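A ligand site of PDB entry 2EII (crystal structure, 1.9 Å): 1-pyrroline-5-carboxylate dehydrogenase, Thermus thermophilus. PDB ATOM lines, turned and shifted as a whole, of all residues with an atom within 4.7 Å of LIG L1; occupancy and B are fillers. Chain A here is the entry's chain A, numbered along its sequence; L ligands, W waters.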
ATOM      1  N   ILE A 180      -6.344 -21.059 -15.875  1.00  0.00           N
ATOM      2  CA  ILE A 180      -5.452 -21.295 -17.002  1.00  0.00           C
ATOM      3  C   ILE A 180      -6.288 -21.231 -18.262  1.00  0.00           C
ATOM      4  O   ILE A 180      -7.197 -22.032 -18.448  1.00  0.00           O
ATOM      5  CB  ILE A 180      -4.736 -22.646 -16.876  1.00  0.00           C
ATOM      6  CG1 ILE A 180      -3.803 -22.641 -15.650  1.00  0.00           C
ATOM      7  CG2 ILE A 180      -3.933 -22.932 -18.134  1.00  0.00           C
ATOM      8  CD1 ILE A 180      -3.225 -24.010 -15.318  1.00  0.00           C
ATOM      9  N   ALA A 181      -5.975 -20.242 -19.102  1.00  0.00           N
ATOM     10  CA  ALA A 181      -6.888 -19.785 -20.139  1.00  0.00           C
ATOM     11  C   ALA A 181      -6.367 -19.987 -21.559  1.00  0.00           C
ATOM     12  O   ALA A 181      -5.153 -20.058 -21.765  1.00  0.00           O
ATOM     13  CB  ALA A 181      -7.245 -18.293 -19.901  1.00  0.00           C
ATOM     14  N   PRO A 182      -7.273 -20.068 -22.549  1.00  0.00           N
ATOM     15  CA  PRO A 182      -6.868 -20.260 -23.944  1.00  0.00           C
ATOM     16  C   PRO A 182      -6.649 -18.946 -24.684  1.00  0.00           C
ATOM     17  O   PRO A 182      -7.069 -17.886 -24.205  1.00  0.00           O
ATOM     18  CB  PRO A 182      -8.077 -21.001 -24.538  1.00  0.00           C
ATOM     19  CG  PRO A 182      -9.246 -20.371 -23.824  1.00  0.00           C
ATOM     20  CD  PRO A 182      -8.738 -20.050 -22.409  1.00  0.00           C
ATOM     21  N   TRP A 183      -6.007 -19.023 -25.852  1.00  0.00           N
ATOM     22  CA  TRP A 183      -5.777 -17.833 -26.701  1.00  0.00           C
ATOM     23  C   TRP A 183      -6.974 -17.441 -27.572  1.00  0.00           C
ATOM     24  O   TRP A 183      -6.998 -16.347 -28.115  1.00  0.00           O
ATOM     25  CB  TRP A 183      -4.535 -18.021 -27.593  1.00  0.00           C
ATOM     26  CG  TRP A 183      -4.548 -19.289 -28.418  1.00  0.00           C
ATOM     27  CD1 TRP A 183      -3.908 -20.453 -28.102  1.00  0.00           C
ATOM     28  CD2 TRP A 183      -5.241 -19.537 -29.648  1.00  0.00           C
ATOM     29  NE1 TRP A 183      -4.161 -21.411 -29.055  1.00  0.00           N
ATOM     30  CE2 TRP A 183      -4.962 -20.867 -30.029  1.00  0.00           C
ATOM     31  CE3 TRP A 183      -6.063 -18.752 -30.490  1.00  0.00           C
ATOM     32  CZ2 TRP A 183      -5.479 -21.457 -31.202  1.00  0.00           C
ATOM     33  CZ3 TRP A 183      -6.565 -19.334 -31.664  1.00  0.00           C
ATOM     34  CH2 TRP A 183      -6.273 -20.665 -32.004  1.00  0.00           C
ATOM     35  N   ASN A 184      -7.957 -18.332 -27.747  1.00  0.00           N
ATOM     36  CA  ASN A 184      -8.994 -18.073 -28.755  1.00  0.00           C
ATOM     37  C   ASN A 184     -10.123 -17.122 -28.338  1.00  0.00           C
ATOM     38  O   ASN A 184     -10.709 -16.469 -29.189  1.00  0.00           O
ATOM     39  CB  ASN A 184      -9.540 -19.379 -29.364  1.00  0.00           C
ATOM     40  CG  ASN A 184     -10.431 -20.153 -28.422  1.00  0.00           C
ATOM     41  OD1 ASN A 184     -10.250 -20.122 -27.203  1.00  0.00           O
ATOM     42  ND2 ASN A 184     -11.399 -20.854 -28.991  1.00  0.00           N
ATOM     43  N   ILE A 189     -13.214 -15.609 -22.177  1.00  0.00           N
ATOM     44  CA  ILE A 189     -13.039 -16.788 -21.303  1.00  0.00           C
ATOM     45  C   ILE A 189     -12.089 -16.524 -20.142  1.00  0.00           C
ATOM     46  O   ILE A 189     -12.314 -16.970 -19.003  1.00  0.00           O
ATOM     47  CB  ILE A 189     -12.655 -18.041 -22.103  1.00  0.00           C
ATOM     48  CG1 ILE A 189     -13.847 -18.492 -22.948  1.00  0.00           C
ATOM     49  CG2 ILE A 189     -12.259 -19.207 -21.166  1.00  0.00           C
ATOM     50  CD1 ILE A 189     -13.514 -19.562 -23.959  1.00  0.00           C
ATOM     51  N   LYS A 207      -3.366 -17.322 -15.457  1.00  0.00           N
ATOM     52  CA  LYS A 207      -2.291 -17.647 -16.376  1.00  0.00           C
ATOM     53  C   LYS A 207      -2.857 -17.549 -17.792  1.00  0.00           C
ATOM     54  O   LYS A 207      -3.481 -18.495 -18.283  1.00  0.00           O
ATOM     55  CB  LYS A 207      -1.761 -19.067 -16.073  1.00  0.00           C
ATOM     56  CG  LYS A 207      -0.255 -19.291 -16.299  1.00  0.00           C
ATOM     57  CD  LYS A 207       0.170 -19.053 -17.753  1.00  0.00           C
ATOM     58  CE  LYS A 207      -0.314 -20.176 -18.696  1.00  0.00           C
ATOM     59  NZ  LYS A 207       0.073 -19.839 -20.108  1.00  0.00           N
ATOM     60  N   PRO A 208      -2.644 -16.398 -18.467  1.00  0.00           N
ATOM     61  CA  PRO A 208      -3.131 -16.231 -19.843  1.00  0.00           C
ATOM     62  C   PRO A 208      -2.356 -17.118 -20.813  1.00  0.00           C
ATOM     63  O   PRO A 208      -1.189 -17.482 -20.530  1.00  0.00           O
ATOM     64  CB  PRO A 208      -2.823 -14.769 -20.152  1.00  0.00           C
ATOM     65  CG  PRO A 208      -1.568 -14.507 -19.346  1.00  0.00           C
ATOM     66  CD  PRO A 208      -1.869 -15.214 -18.031  1.00  0.00           C
ATOM     67  N   ALA A 209      -2.970 -17.426 -21.948  1.00  0.00           N
ATOM     68  CA  ALA A 209      -2.286 -18.167 -22.987  1.00  0.00           C
ATOM     69  C   ALA A 209      -1.153 -17.313 -23.558  1.00  0.00           C
ATOM     70  O   ALA A 209      -1.269 -16.080 -23.650  1.00  0.00           O
ATOM     71  CB  ALA A 209      -3.258 -18.580 -24.089  1.00  0.00           C
ATOM     72  N   GLU A 210      -0.062 -17.975 -23.914  1.00  0.00           N
ATOM     73  CA  GLU A 210       1.131 -17.304 -24.467  1.00  0.00           C
ATOM     74  C   GLU A 210       0.837 -16.356 -25.638  1.00  0.00           C
ATOM     75  O   GLU A 210       1.428 -15.269 -25.727  1.00  0.00           O
ATOM     76  CB  GLU A 210       2.149 -18.370 -24.904  1.00  0.00           C
ATOM     77  CG  GLU A 210       2.749 -19.138 -23.722  1.00  0.00           C
ATOM     78  CD  GLU A 210       2.041 -20.444 -23.383  1.00  0.00           C
ATOM     79  OE1 GLU A 210       0.792 -20.565 -23.484  1.00  0.00           O
ATOM     80  OE2 GLU A 210       2.765 -21.391 -23.000  1.00  0.00           O
ATOM     81  N   GLY A 238       3.116 -16.572 -18.798  1.00  0.00           N
ATOM     82  CA  GLY A 238       4.219 -17.540 -18.700  1.00  0.00           C
ATOM     83  C   GLY A 238       3.914 -18.773 -19.506  1.00  0.00           C
ATOM     84  O   GLY A 238       2.857 -18.847 -20.169  1.00  0.00           O
ATOM     85  N   VAL A 239       4.824 -19.744 -19.467  1.00  0.00           N
ATOM     86  CA  VAL A 239       4.710 -20.976 -20.242  1.00  0.00           C
ATOM     87  C   VAL A 239       3.814 -21.981 -19.537  1.00  0.00           C
ATOM     88  O   VAL A 239       4.049 -22.301 -18.370  1.00  0.00           O
ATOM     89  CB  VAL A 239       6.111 -21.607 -20.495  1.00  0.00           C
ATOM     90  CG1 VAL A 239       5.993 -22.922 -21.258  1.00  0.00           C
ATOM     91  CG2 VAL A 239       6.972 -20.616 -21.274  1.00  0.00           C
ATOM     92  N   GLY A 240       2.811 -22.476 -20.256  1.00  0.00           N
ATOM     93  CA  GLY A 240       1.824 -23.378 -19.640  1.00  0.00           C
ATOM     94  C   GLY A 240       2.434 -24.590 -18.977  1.00  0.00           C
ATOM     95  O   GLY A 240       2.115 -24.906 -17.828  1.00  0.00           O
ATOM     96  N   GLU A 241       3.326 -25.266 -19.705  1.00  0.00           N
ATOM     97  CA  GLU A 241       3.969 -26.476 -19.188  1.00  0.00           C
ATOM     98  C   GLU A 241       4.960 -26.212 -18.080  1.00  0.00           C
ATOM     99  O   GLU A 241       5.481 -27.154 -17.479  1.00  0.00           O
ATOM    100  CB  GLU A 241       4.678 -27.221 -20.315  1.00  0.00           C
ATOM    101  CG  GLU A 241       3.730 -27.918 -21.242  1.00  0.00           C
ATOM    102  CD  GLU A 241       4.427 -28.562 -22.422  1.00  0.00           C
ATOM    103  OE1 GLU A 241       5.667 -28.397 -22.564  1.00  0.00           O
ATOM    104  OE2 GLU A 241       3.733 -29.237 -23.204  1.00  0.00           O
ATOM    105  N   GLY A 244       2.246 -22.926 -15.407  1.00  0.00           N
ATOM    106  CA  GLY A 244       0.887 -23.515 -15.375  1.00  0.00           C
ATOM    107  C   GLY A 244       0.889 -24.854 -14.641  1.00  0.00           C
ATOM    108  O   GLY A 244       0.150 -25.047 -13.664  1.00  0.00           O
ATOM    109  N   ALA A 245       1.726 -25.784 -15.102  1.00  0.00           N
ATOM    110  CA  ALA A 245       1.839 -27.105 -14.464  1.00  0.00           C
ATOM    111  C   ALA A 245       2.284 -26.995 -13.012  1.00  0.00           C
ATOM    112  O   ALA A 245       1.809 -27.742 -12.147  1.00  0.00           O
ATOM    113  CB  ALA A 245       2.796 -28.011 -15.251  1.00  0.00           C
ATOM    114  N   VAL A 248      -0.848 -26.093 -11.070  1.00  0.00           N
ATOM    115  CA  VAL A 248      -1.747 -27.257 -11.068  1.00  0.00           C
ATOM    116  C   VAL A 248      -1.326 -28.315 -10.025  1.00  0.00           C
ATOM    117  O   VAL A 248      -2.147 -28.817  -9.253  1.00  0.00           O
ATOM    118  CB  VAL A 248      -1.856 -27.880 -12.499  1.00  0.00           C
ATOM    119  CG1 VAL A 248      -2.527 -29.247 -12.460  1.00  0.00           C
ATOM    120  CG2 VAL A 248      -2.623 -26.941 -13.425  1.00  0.00           C
ATOM    121  N   PHE A 258      -9.772 -24.437 -15.842  1.00  0.00           N
ATOM    122  CA  PHE A 258      -9.029 -24.592 -17.093  1.00  0.00           C
ATOM    123  C   PHE A 258      -9.952 -24.606 -18.284  1.00  0.00           C
ATOM    124  O   PHE A 258     -10.967 -25.286 -18.274  1.00  0.00           O
ATOM    125  CB  PHE A 258      -8.229 -25.908 -17.098  1.00  0.00           C
ATOM    126  CG  PHE A 258      -7.595 -26.215 -18.424  1.00  0.00           C
ATOM    127  CD1 PHE A 258      -6.391 -25.572 -18.799  1.00  0.00           C
ATOM    128  CD2 PHE A 258      -8.185 -27.121 -19.318  1.00  0.00           C
ATOM    129  CE1 PHE A 258      -5.807 -25.832 -20.037  1.00  0.00           C
ATOM    130  CE2 PHE A 258      -7.609 -27.378 -20.556  1.00  0.00           C
ATOM    131  CZ  PHE A 258      -6.406 -26.739 -20.909  1.00  0.00           C
ATOM    132  N   THR A 259      -9.577 -23.859 -19.310  1.00  0.00           N
ATOM    133  CA  THR A 259     -10.191 -24.043 -20.621  1.00  0.00           C
ATOM    134  C   THR A 259      -9.071 -24.135 -21.671  1.00  0.00           C
ATOM    135  O   THR A 259      -8.142 -23.335 -21.664  1.00  0.00           O
ATOM    136  CB  THR A 259     -11.140 -22.877 -20.950  1.00  0.00           C
ATOM    137  OG1 THR A 259     -12.188 -22.833 -19.970  1.00  0.00           O
ATOM    138  CG2 THR A 259     -11.761 -23.064 -22.333  1.00  0.00           C
ATOM    139  N   GLY A 260      -9.151 -25.140 -22.531  1.00  0.00           N
ATOM    140  CA  GLY A 260      -8.080 -25.373 -23.497  1.00  0.00           C
ATOM    141  C   GLY A 260      -8.192 -26.736 -24.166  1.00  0.00           C
ATOM    142  O   GLY A 260      -9.301 -27.295 -24.245  1.00  0.00           O
ATOM    143  N   SER A 261      -7.075 -27.251 -24.660  1.00  0.00           N
ATOM    144  CA  SER A 261      -7.077 -28.480 -25.438  1.00  0.00           C
ATOM    145  C   SER A 261      -7.367 -29.686 -24.554  1.00  0.00           C
ATOM    146  O   SER A 261      -7.046 -29.683 -23.355  1.00  0.00           O
ATOM    147  CB  SER A 261      -5.727 -28.706 -26.119  1.00  0.00           C
ATOM    148  OG  SER A 261      -4.725 -28.943 -25.129  1.00  0.00           O
ATOM    149  N   LEU A 262      -7.978 -30.710 -25.142  1.00  0.00           N
ATOM    150  CA  LEU A 262      -8.137 -32.004 -24.473  1.00  0.00           C
ATOM    151  C   LEU A 262      -6.798 -32.558 -23.948  1.00  0.00           C
ATOM    152  O   LEU A 262      -6.724 -33.049 -22.822  1.00  0.00           O
ATOM    153  CB  LEU A 262      -8.810 -33.009 -25.418  1.00  0.00           C
ATOM    154  CG  LEU A 262      -9.021 -34.441 -24.886  1.00  0.00           C
ATOM    155  CD1 LEU A 262      -9.783 -34.432 -23.547  1.00  0.00           C
ATOM    156  CD2 LEU A 262      -9.717 -35.317 -25.907  1.00  0.00           C
ATOM    157  N   VAL A 264      -4.045 -31.172 -22.880  1.00  0.00           N
ATOM    158  CA  VAL A 264      -3.685 -30.503 -21.639  1.00  0.00           C
ATOM    159  C   VAL A 264      -4.723 -30.740 -20.525  1.00  0.00           C
ATOM    160  O   VAL A 264      -4.357 -31.036 -19.379  1.00  0.00           O
ATOM    161  CB  VAL A 264      -3.400 -28.984 -21.869  1.00  0.00           C
ATOM    162  CG1 VAL A 264      -3.203 -28.277 -20.529  1.00  0.00           C
ATOM    163  CG2 VAL A 264      -2.117 -28.805 -22.734  1.00  0.00           C
ATOM    164  N   LYS A 267      -4.105 -34.052 -18.707  1.00  0.00           N
ATOM    165  CA  LYS A 267      -3.001 -33.948 -17.744  1.00  0.00           C
ATOM    166  C   LYS A 267      -3.398 -33.222 -16.461  1.00  0.00           C
ATOM    167  O   LYS A 267      -3.021 -33.629 -15.361  1.00  0.00           O
ATOM    168  CB  LYS A 267      -1.807 -33.214 -18.379  1.00  0.00           C
ATOM    169  CG  LYS A 267      -1.235 -33.957 -19.570  1.00  0.00           C
ATOM    170  CD  LYS A 267      -0.078 -33.184 -20.210  1.00  0.00           C
ATOM    171  CE  LYS A 267       0.344 -33.876 -21.511  1.00  0.00           C
ATOM    172  NZ  LYS A 267       1.460 -33.139 -22.167  1.00  0.00           N
ATOM    173  N   ILE A 268      -4.142 -32.143 -16.614  1.00  0.00           N
ATOM    174  CA  ILE A 268      -4.559 -31.319 -15.469  1.00  0.00           C
ATOM    175  C   ILE A 268      -5.545 -32.077 -14.569  1.00  0.00           C
ATOM    176  O   ILE A 268      -5.394 -32.063 -13.347  1.00  0.00           O
ATOM    177  CB  ILE A 268      -5.173 -30.003 -15.959  1.00  0.00           C
ATOM    178  CG1 ILE A 268      -4.060 -29.100 -16.523  1.00  0.00           C
ATOM    179  CG2 ILE A 268      -5.951 -29.307 -14.866  1.00  0.00           C
ATOM    180  CD1 ILE A 268      -4.578 -27.817 -17.141  1.00  0.00           C
ATOM    181  N   GLU A 288     -12.563 -27.524 -19.411  1.00  0.00           N
ATOM    182  CA  GLU A 288     -13.477 -27.433 -20.529  1.00  0.00           C
ATOM    183  C   GLU A 288     -12.568 -27.523 -21.757  1.00  0.00           C
ATOM    184  O   GLU A 288     -11.663 -26.693 -21.957  1.00  0.00           O
ATOM    185  CB  GLU A 288     -14.336 -26.171 -20.388  1.00  0.00           C
ATOM    186  CG  GLU A 288     -15.108 -26.140 -19.021  1.00  0.00           C
ATOM    187  CD  GLU A 288     -16.078 -27.346 -18.812  1.00  0.00           C
ATOM    188  OE1 GLU A 288     -16.729 -27.760 -19.767  1.00  0.00           O
ATOM    189  OE2 GLU A 288     -16.181 -27.881 -17.694  1.00  0.00           O
ATOM    190  N   THR A 289     -12.778 -28.584 -22.517  1.00  0.00           N
ATOM    191  CA  THR A 289     -11.800 -29.039 -23.478  1.00  0.00           C
ATOM    192  C   THR A 289     -12.429 -28.870 -24.855  1.00  0.00           C
ATOM    193  O   THR A 289     -13.379 -28.109 -25.008  1.00  0.00           O
ATOM    194  CB  THR A 289     -11.361 -30.493 -23.149  1.00  0.00           C
ATOM    195  OG1 THR A 289     -12.511 -31.280 -22.780  1.00  0.00           O
ATOM    196  CG2 THR A 289     -10.389 -30.494 -21.955  1.00  0.00           C
ATOM    197  N   GLY A 290     -11.925 -29.572 -25.865  1.00  0.00           N
ATOM    198  CA  GLY A 290     -12.368 -29.268 -27.224  1.00  0.00           C
ATOM    199  C   GLY A 290     -13.685 -29.887 -27.636  1.00  0.00           C
ATOM    200  O   GLY A 290     -14.412 -30.477 -26.840  1.00  0.00           O
ATOM    201  N   GLY A 291     -13.980 -29.730 -28.910  1.00  0.00           N
ATOM    202  CA  GLY A 291     -15.092 -30.470 -29.527  1.00  0.00           C
ATOM    203  C   GLY A 291     -14.777 -30.903 -30.930  1.00  0.00           C
ATOM    204  O   GLY A 291     -13.770 -30.484 -31.503  1.00  0.00           O
ATOM    205  N   CYS A 322     -13.937 -23.777 -29.983  1.00  0.00           N
ATOM    206  CA  CYS A 322     -14.319 -25.076 -29.462  1.00  0.00           C
ATOM    207  C   CYS A 322     -15.731 -25.443 -29.913  1.00  0.00           C
ATOM    208  O   CYS A 322     -16.082 -26.613 -29.950  1.00  0.00           O
ATOM    209  CB  CYS A 322     -14.247 -25.062 -27.962  1.00  0.00           C
ATOM    210  SG  CYS A 322     -15.223 -23.724 -27.166  1.00  0.00           S
ATOM    211  N   GLU A 417      -9.785 -32.817 -33.342  1.00  0.00           N
ATOM    212  CA  GLU A 417     -10.039 -31.362 -33.418  1.00  0.00           C
ATOM    213  C   GLU A 417      -8.886 -30.657 -34.140  1.00  0.00           C
ATOM    214  O   GLU A 417      -7.762 -30.581 -33.626  1.00  0.00           O
ATOM    215  CB  GLU A 417     -10.267 -30.790 -32.023  1.00  0.00           C
ATOM    216  CG  GLU A 417     -10.635 -29.308 -32.033  1.00  0.00           C
ATOM    217  CD  GLU A 417     -10.766 -28.742 -30.640  1.00  0.00           C
ATOM    218  OE1 GLU A 417     -11.784 -28.069 -30.397  1.00  0.00           O
ATOM    219  OE2 GLU A 417      -9.860 -28.971 -29.791  1.00  0.00           O
ATOM    220  N   PHE A 419      -9.123 -27.356 -35.368  1.00  0.00           N
ATOM    221  CA  PHE A 419      -9.072 -25.980 -34.865  1.00  0.00           C
ATOM    222  C   PHE A 419      -8.570 -24.982 -35.915  1.00  0.00           C
ATOM    223  O   PHE A 419      -7.783 -24.081 -35.609  1.00  0.00           O
ATOM    224  CB  PHE A 419      -8.222 -25.901 -33.578  1.00  0.00           C
ATOM    225  CG  PHE A 419      -8.841 -25.052 -32.501  1.00  0.00           C
ATOM    226  CD1 PHE A 419      -8.219 -23.890 -32.049  1.00  0.00           C
ATOM    227  CD2 PHE A 419     -10.061 -25.429 -31.931  1.00  0.00           C
ATOM    228  CE1 PHE A 419      -8.820 -23.106 -31.055  1.00  0.00           C
ATOM    229  CE2 PHE A 419     -10.658 -24.661 -30.937  1.00  0.00           C
ATOM    230  CZ  PHE A 419     -10.025 -23.497 -30.493  1.00  0.00           C
ATOM    231  N   LEU A 445     -19.615 -31.274 -27.360  1.00  0.00           N
ATOM    232  CA  LEU A 445     -19.675 -29.852 -26.998  1.00  0.00           C
ATOM    233  C   LEU A 445     -20.845 -29.130 -27.639  1.00  0.00           C
ATOM    234  O   LEU A 445     -21.820 -28.841 -26.941  1.00  0.00           O
ATOM    235  CB  LEU A 445     -18.324 -29.106 -27.221  1.00  0.00           C
ATOM    236  CG  LEU A 445     -18.230 -27.672 -26.647  1.00  0.00           C
ATOM    237  CD1 LEU A 445     -18.793 -27.560 -25.219  1.00  0.00           C
ATOM    238  CD2 LEU A 445     -16.769 -27.194 -26.683  1.00  0.00           C
ATOM    239  N   PHE A 485     -23.084 -22.682 -21.164  1.00  0.00           N
ATOM    240  CA  PHE A 485     -22.132 -23.265 -22.115  1.00  0.00           C
ATOM    241  C   PHE A 485     -21.185 -24.293 -21.494  1.00  0.00           C
ATOM    242  O   PHE A 485     -20.500 -24.025 -20.514  1.00  0.00           O
ATOM    243  CB  PHE A 485     -21.328 -22.171 -22.830  1.00  0.00           C
ATOM    244  CG  PHE A 485     -20.459 -22.716 -23.946  1.00  0.00           C
ATOM    245  CD1 PHE A 485     -21.016 -23.029 -25.186  1.00  0.00           C
ATOM    246  CD2 PHE A 485     -19.101 -22.971 -23.730  1.00  0.00           C
ATOM    247  CE1 PHE A 485     -20.227 -23.545 -26.225  1.00  0.00           C
ATOM    248  CE2 PHE A 485     -18.299 -23.508 -24.755  1.00  0.00           C
ATOM    249  CZ  PHE A 485     -18.851 -23.784 -26.004  1.00  0.00           C
ATOM    250  N   SER A 491     -15.359 -33.400 -24.080  1.00  0.00           N
ATOM    251  CA  SER A 491     -15.441 -31.937 -24.137  1.00  0.00           C
ATOM    252  C   SER A 491     -15.356 -31.285 -22.755  1.00  0.00           C
ATOM    253  O   SER A 491     -15.334 -30.050 -22.647  1.00  0.00           O
ATOM    254  CB  SER A 491     -16.716 -31.496 -24.875  1.00  0.00           C
ATOM    255  OG  SER A 491     -16.617 -31.874 -26.246  1.00  0.00           O
HETATM  256  P1  LIG L   1      -3.880 -25.348 -24.805  1.00  0.00           P
HETATM  257  O1  LIG L   1      -2.741 -25.589 -25.692  1.00  0.00           O
HETATM  258  O2  LIG L   1      -4.337 -26.554 -24.076  1.00  0.00           O
HETATM  259  O3  LIG L   1      -3.464 -24.250 -23.719  1.00  0.00           O
HETATM  260  C1  LIG L   1      -4.439 -23.622 -22.909  1.00  0.00           C
HETATM  261  C2  LIG L   1      -3.742 -23.009 -21.691  1.00  0.00           C
HETATM  262  O4  LIG L   1      -3.068 -24.044 -20.986  1.00  0.00           O
HETATM  263  C3  LIG L   1      -2.656 -22.000 -22.087  1.00  0.00           C
HETATM  264  O5  LIG L   1      -2.668 -21.002 -21.089  1.00  0.00           O
HETATM  265  C4  LIG L   1      -1.341 -22.777 -21.983  1.00  0.00           C
HETATM  266  O6  LIG L   1      -0.191 -21.999 -21.690  1.00  0.00           O
HETATM  267  C5  LIG L   1      -1.693 -23.709 -20.822  1.00  0.00           C
HETATM  268  N1  LIG L   1      -0.959 -24.983 -20.787  1.00  0.00           N
HETATM  269  C6  LIG L   1      -0.365 -25.677 -21.841  1.00  0.00           C
HETATM  270  N2  LIG L   1       0.166 -26.820 -21.330  1.00  0.00           N
HETATM  271  C7  LIG L   1      -0.075 -26.857 -19.990  1.00  0.00           C
HETATM  272  C8  LIG L   1       0.231 -27.779 -18.978  1.00  0.00           C
HETATM  273  N3  LIG L   1       0.831 -28.939 -19.234  1.00  0.00           N
HETATM  274  N4  LIG L   1      -0.170 -27.512 -17.694  1.00  0.00           N
HETATM  275  C9  LIG L   1      -0.868 -26.361 -17.356  1.00  0.00           C
HETATM  276  N5  LIG L   1      -1.173 -25.462 -18.360  1.00  0.00           N
HETATM  277  C10 LIG L   1      -0.793 -25.703 -19.643  1.00  0.00           C
HETATM  278  O7  LIG L   1      -5.145 -24.759 -25.594  1.00  0.00           O
HETATM  279  P2  LIG L   1      -5.170 -23.437 -26.532  1.00  0.00           P
HETATM  280  O8  LIG L   1      -4.841 -22.218 -25.756  1.00  0.00           O
HETATM  281  O9  LIG L   1      -4.418 -23.790 -27.768  1.00  0.00           O
HETATM  282  O10 LIG L   1      -6.730 -23.359 -26.884  1.00  0.00           O
HETATM  283  C11 LIG L   1      -7.276 -24.150 -27.923  1.00  0.00           C
HETATM  284  C12 LIG L   1      -8.103 -25.257 -27.291  1.00  0.00           C
HETATM  285  O11 LIG L   1      -8.991 -24.679 -26.338  1.00  0.00           O
HETATM  286  C13 LIG L   1      -8.978 -26.001 -28.287  1.00  0.00           C
HETATM  287  O12 LIG L   1      -8.860 -27.383 -28.102  1.00  0.00           O
HETATM  288  C14 LIG L   1     -10.374 -25.570 -27.890  1.00  0.00           C
HETATM  289  O13 LIG L   1     -11.380 -26.510 -28.202  1.00  0.00           O
HETATM  290  C15 LIG L   1     -10.228 -25.325 -26.394  1.00  0.00           C
HETATM  291  N6  LIG L   1     -11.315 -24.477 -25.954  1.00  0.00           N
HETATM  292  C16 LIG L   1     -12.374 -25.063 -25.333  1.00  0.00           C
HETATM  293  C17 LIG L   1     -13.450 -24.279 -24.941  1.00  0.00           C
HETATM  294  C18 LIG L   1     -14.503 -24.826 -24.037  1.00  0.00           C
HETATM  295  O14 LIG L   1     -15.290 -23.892 -23.375  1.00  0.00           O
HETATM  296  N7  LIG L   1     -14.696 -26.137 -23.876  1.00  0.00           N
HETATM  297  C19 LIG L   1     -13.420 -22.902 -25.190  1.00  0.00           C
HETATM  298  C20 LIG L   1     -12.317 -22.314 -25.822  1.00  0.00           C
HETATM  299  C21 LIG L   1     -11.261 -23.119 -26.211  1.00  0.00           C
HETATM  300  N1  LG2 L   2     -19.461 -18.463 -26.357  1.00  0.00           N
HETATM  301  C1  LG2 L   2     -18.542 -18.707 -27.522  1.00  0.00           C
HETATM  302  C2  LG2 L   2     -19.140 -19.712 -28.510  1.00  0.00           C
HETATM  303  O1  LG2 L   2     -20.096 -20.458 -28.168  1.00  0.00           O
HETATM  304  C3  LG2 L   2     -17.105 -19.158 -27.083  1.00  0.00           C
HETATM  305  C4  LG2 L   2     -16.563 -18.270 -25.955  1.00  0.00           C
HETATM  306  C5  LG2 L   2     -17.071 -20.636 -26.672  1.00  0.00           C
HETATM  307  O2  LG2 L   2     -18.670 -19.780 -29.668  1.00  0.00           O
HETATM  308  O   HOH W   1     -16.863 -27.841 -22.296  1.00  0.00           O
HETATM  309  O   HOH W   2       1.267 -28.026 -23.517  1.00  0.00           O
HETATM  310  O   HOH W   3      -1.844 -21.663 -25.417  1.00  0.00           O
HETATM  311  O   HOH W   4      -0.310 -27.472 -25.634  1.00  0.00           O
HETATM  312  O   HOH W   5      -9.422 -30.783 -27.781  1.00  0.00           O
HETATM  313  O   HOH W   6       1.526 -30.047 -21.700  1.00  0.00           O
HETATM  314  O   HOH W   7     -14.227 -21.718 -28.214  1.00  0.00           O
HETATM  315  O   HOH W   8      -1.925 -23.968 -27.806  1.00  0.00           O
HETATM  316  O   HOH W   9      -6.249 -27.461 -29.587  1.00  0.00           O
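OE1 of Glu 210 lies within hydrogen-bond range of O6 of LIG L1, 2.5 Å away. O12 of LIG L1 is in hydrogen-bond range of OE2 of Glu 417, 2.5 Å away. The backbone carbonyl oxygen (O) of Thr 289 lies within hydrogen-bond range of a nitrogen (N7) of LIG L1 (2.6 Å). The backbone NH (N) of Ser 261 sits at hydrogen-bond distance from an oxygen (O2) of LIG L1, 2.9 Å away. O2 of LIG L1 sits at hydrogen-bond distance from OG of Ser 261, at 2.6 Å. The side-chain amino group (NZ) of Lys 207 sits at hydrogen-bond distance from an oxygen (O6) of LIG L1, 2.7 Å away. An oxygen (O8) of LIG L1 sits close to the backbone NH (N) of Trp 183 (3.4 Å). NE1 of Trp 183 sits at hydrogen-bond distance from O9 of LIG L1 (2.7 Å). The backbone carbonyl oxygen (O) of Ala 181 lies within hydrogen-bond range of an oxygen (O5) of LIG L1, at 2.7 Å. SG of Cys 322 sits close to O14 of LIG L1 (3.8 Å). N of Gly 240 lies close to O6 of LIG L1 (3.4 Å).
The side-chain carboxylate (OE1) of Glu 417 lies within hydrogen-bond range of the backbone NH (N) of Gly 291, at 3.1 Å. NZ of Lys 207 lies within hydrogen-bond range of O of Gly 238 (3.0 Å). The backbone carbonyl oxygen of Ala 181 lies close to the backbone NH of Ala 209 (3.4 Å). N of Gly 260 is in hydrogen-bond range of O of Glu 288 (3.0 Å). The backbone carbonyl oxygen (O) of Gly 290 lies within hydrogen-bond range of the side-chain hydroxyl (OG) of Ser 491 (2.7 Å). The backbone carbonyl oxygen of Ile 180 is in hydrogen-bond range of the backbone NH of Thr 259, at 3.1 Å. N of Glu 288 is in hydrogen-bond range of O of Phe 258 (3.0 Å). The backbone NH of Leu 445 lies within hydrogen-bond range of the side-chain hydroxyl of Ser 491, at 3.3 Å.
The backbone carbonyl oxygen (O) of Gly 260 sits close to an oxygen (O11) of LIG L1 (3.4 Å). Residues that only touch LIG L1: Gly 290 (3.1 Å), Ile 180 (3.2 Å), Phe 419 (3.2 Å), Glu 288 (3.3 Å), Thr 259 (3.3 Å), Asn 184 (3.3 Å), Phe 485 (3.3 Å), Val 264 (3.3 Å), Pro 182 (3.4 Å), Phe 258 (3.4 Å), Ala 209 (3.4 Å), Ala 245 (3.5 Å), Ile 189 (3.5 Å), Gly 244 (3.6 Å), Leu 445 (3.6 Å), Glu 241 (3.7 Å), Pro 208 (3.9 Å) and Ile 268 (3.99 Å). Hydrophobic or aromatic side chains within 4 Å of LIG L1: Ile 180, Pro 182, Trp 183, Ile 189, Ala 209, Ala 245, Phe 258, Val 264, Ile 268, Phe 419, Leu 445 and Phe 485. The nearest printed residue that does not touch LIG L1 is Ser 491 (4.2 Å).
Water W2 lies within hydrogen-bond range of a nitrogen (N2) of LIG L1 and the side-chain carboxylate of Glu 241. Water W6 lies within hydrogen-bond range of OE2 of Glu 241 (2.8 Å), N3 of LIG L1 (2.8 Å) and NZ of Lys 267 (3.1 Å). Water W3 lies within hydrogen-bond range of an oxygen (O8) of LIG L1 and the side-chain carboxylate (OE1) of Glu 210. Water W7 lies within hydrogen-bond range of the side-chain sulfur (SG) of Cys 322 (2.5 Å) and the side-chain amide nitrogen (ND2) of Asn 184 (3.1 Å). Water W1 lies within hydrogen-bond range of OE1 of Glu 288, O of Ser 491 and N7 of LIG L1. Water W5 lies within hydrogen-bond range of the side-chain carboxylate (OE2) of Glu 417 (2.7 Å), the backbone NH (N) of Leu 262 (3.0 Å), the backbone NH (N) of Gly 290 (3.4 Å) and an oxygen (O12) of LIG L1 (3.5 Å).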
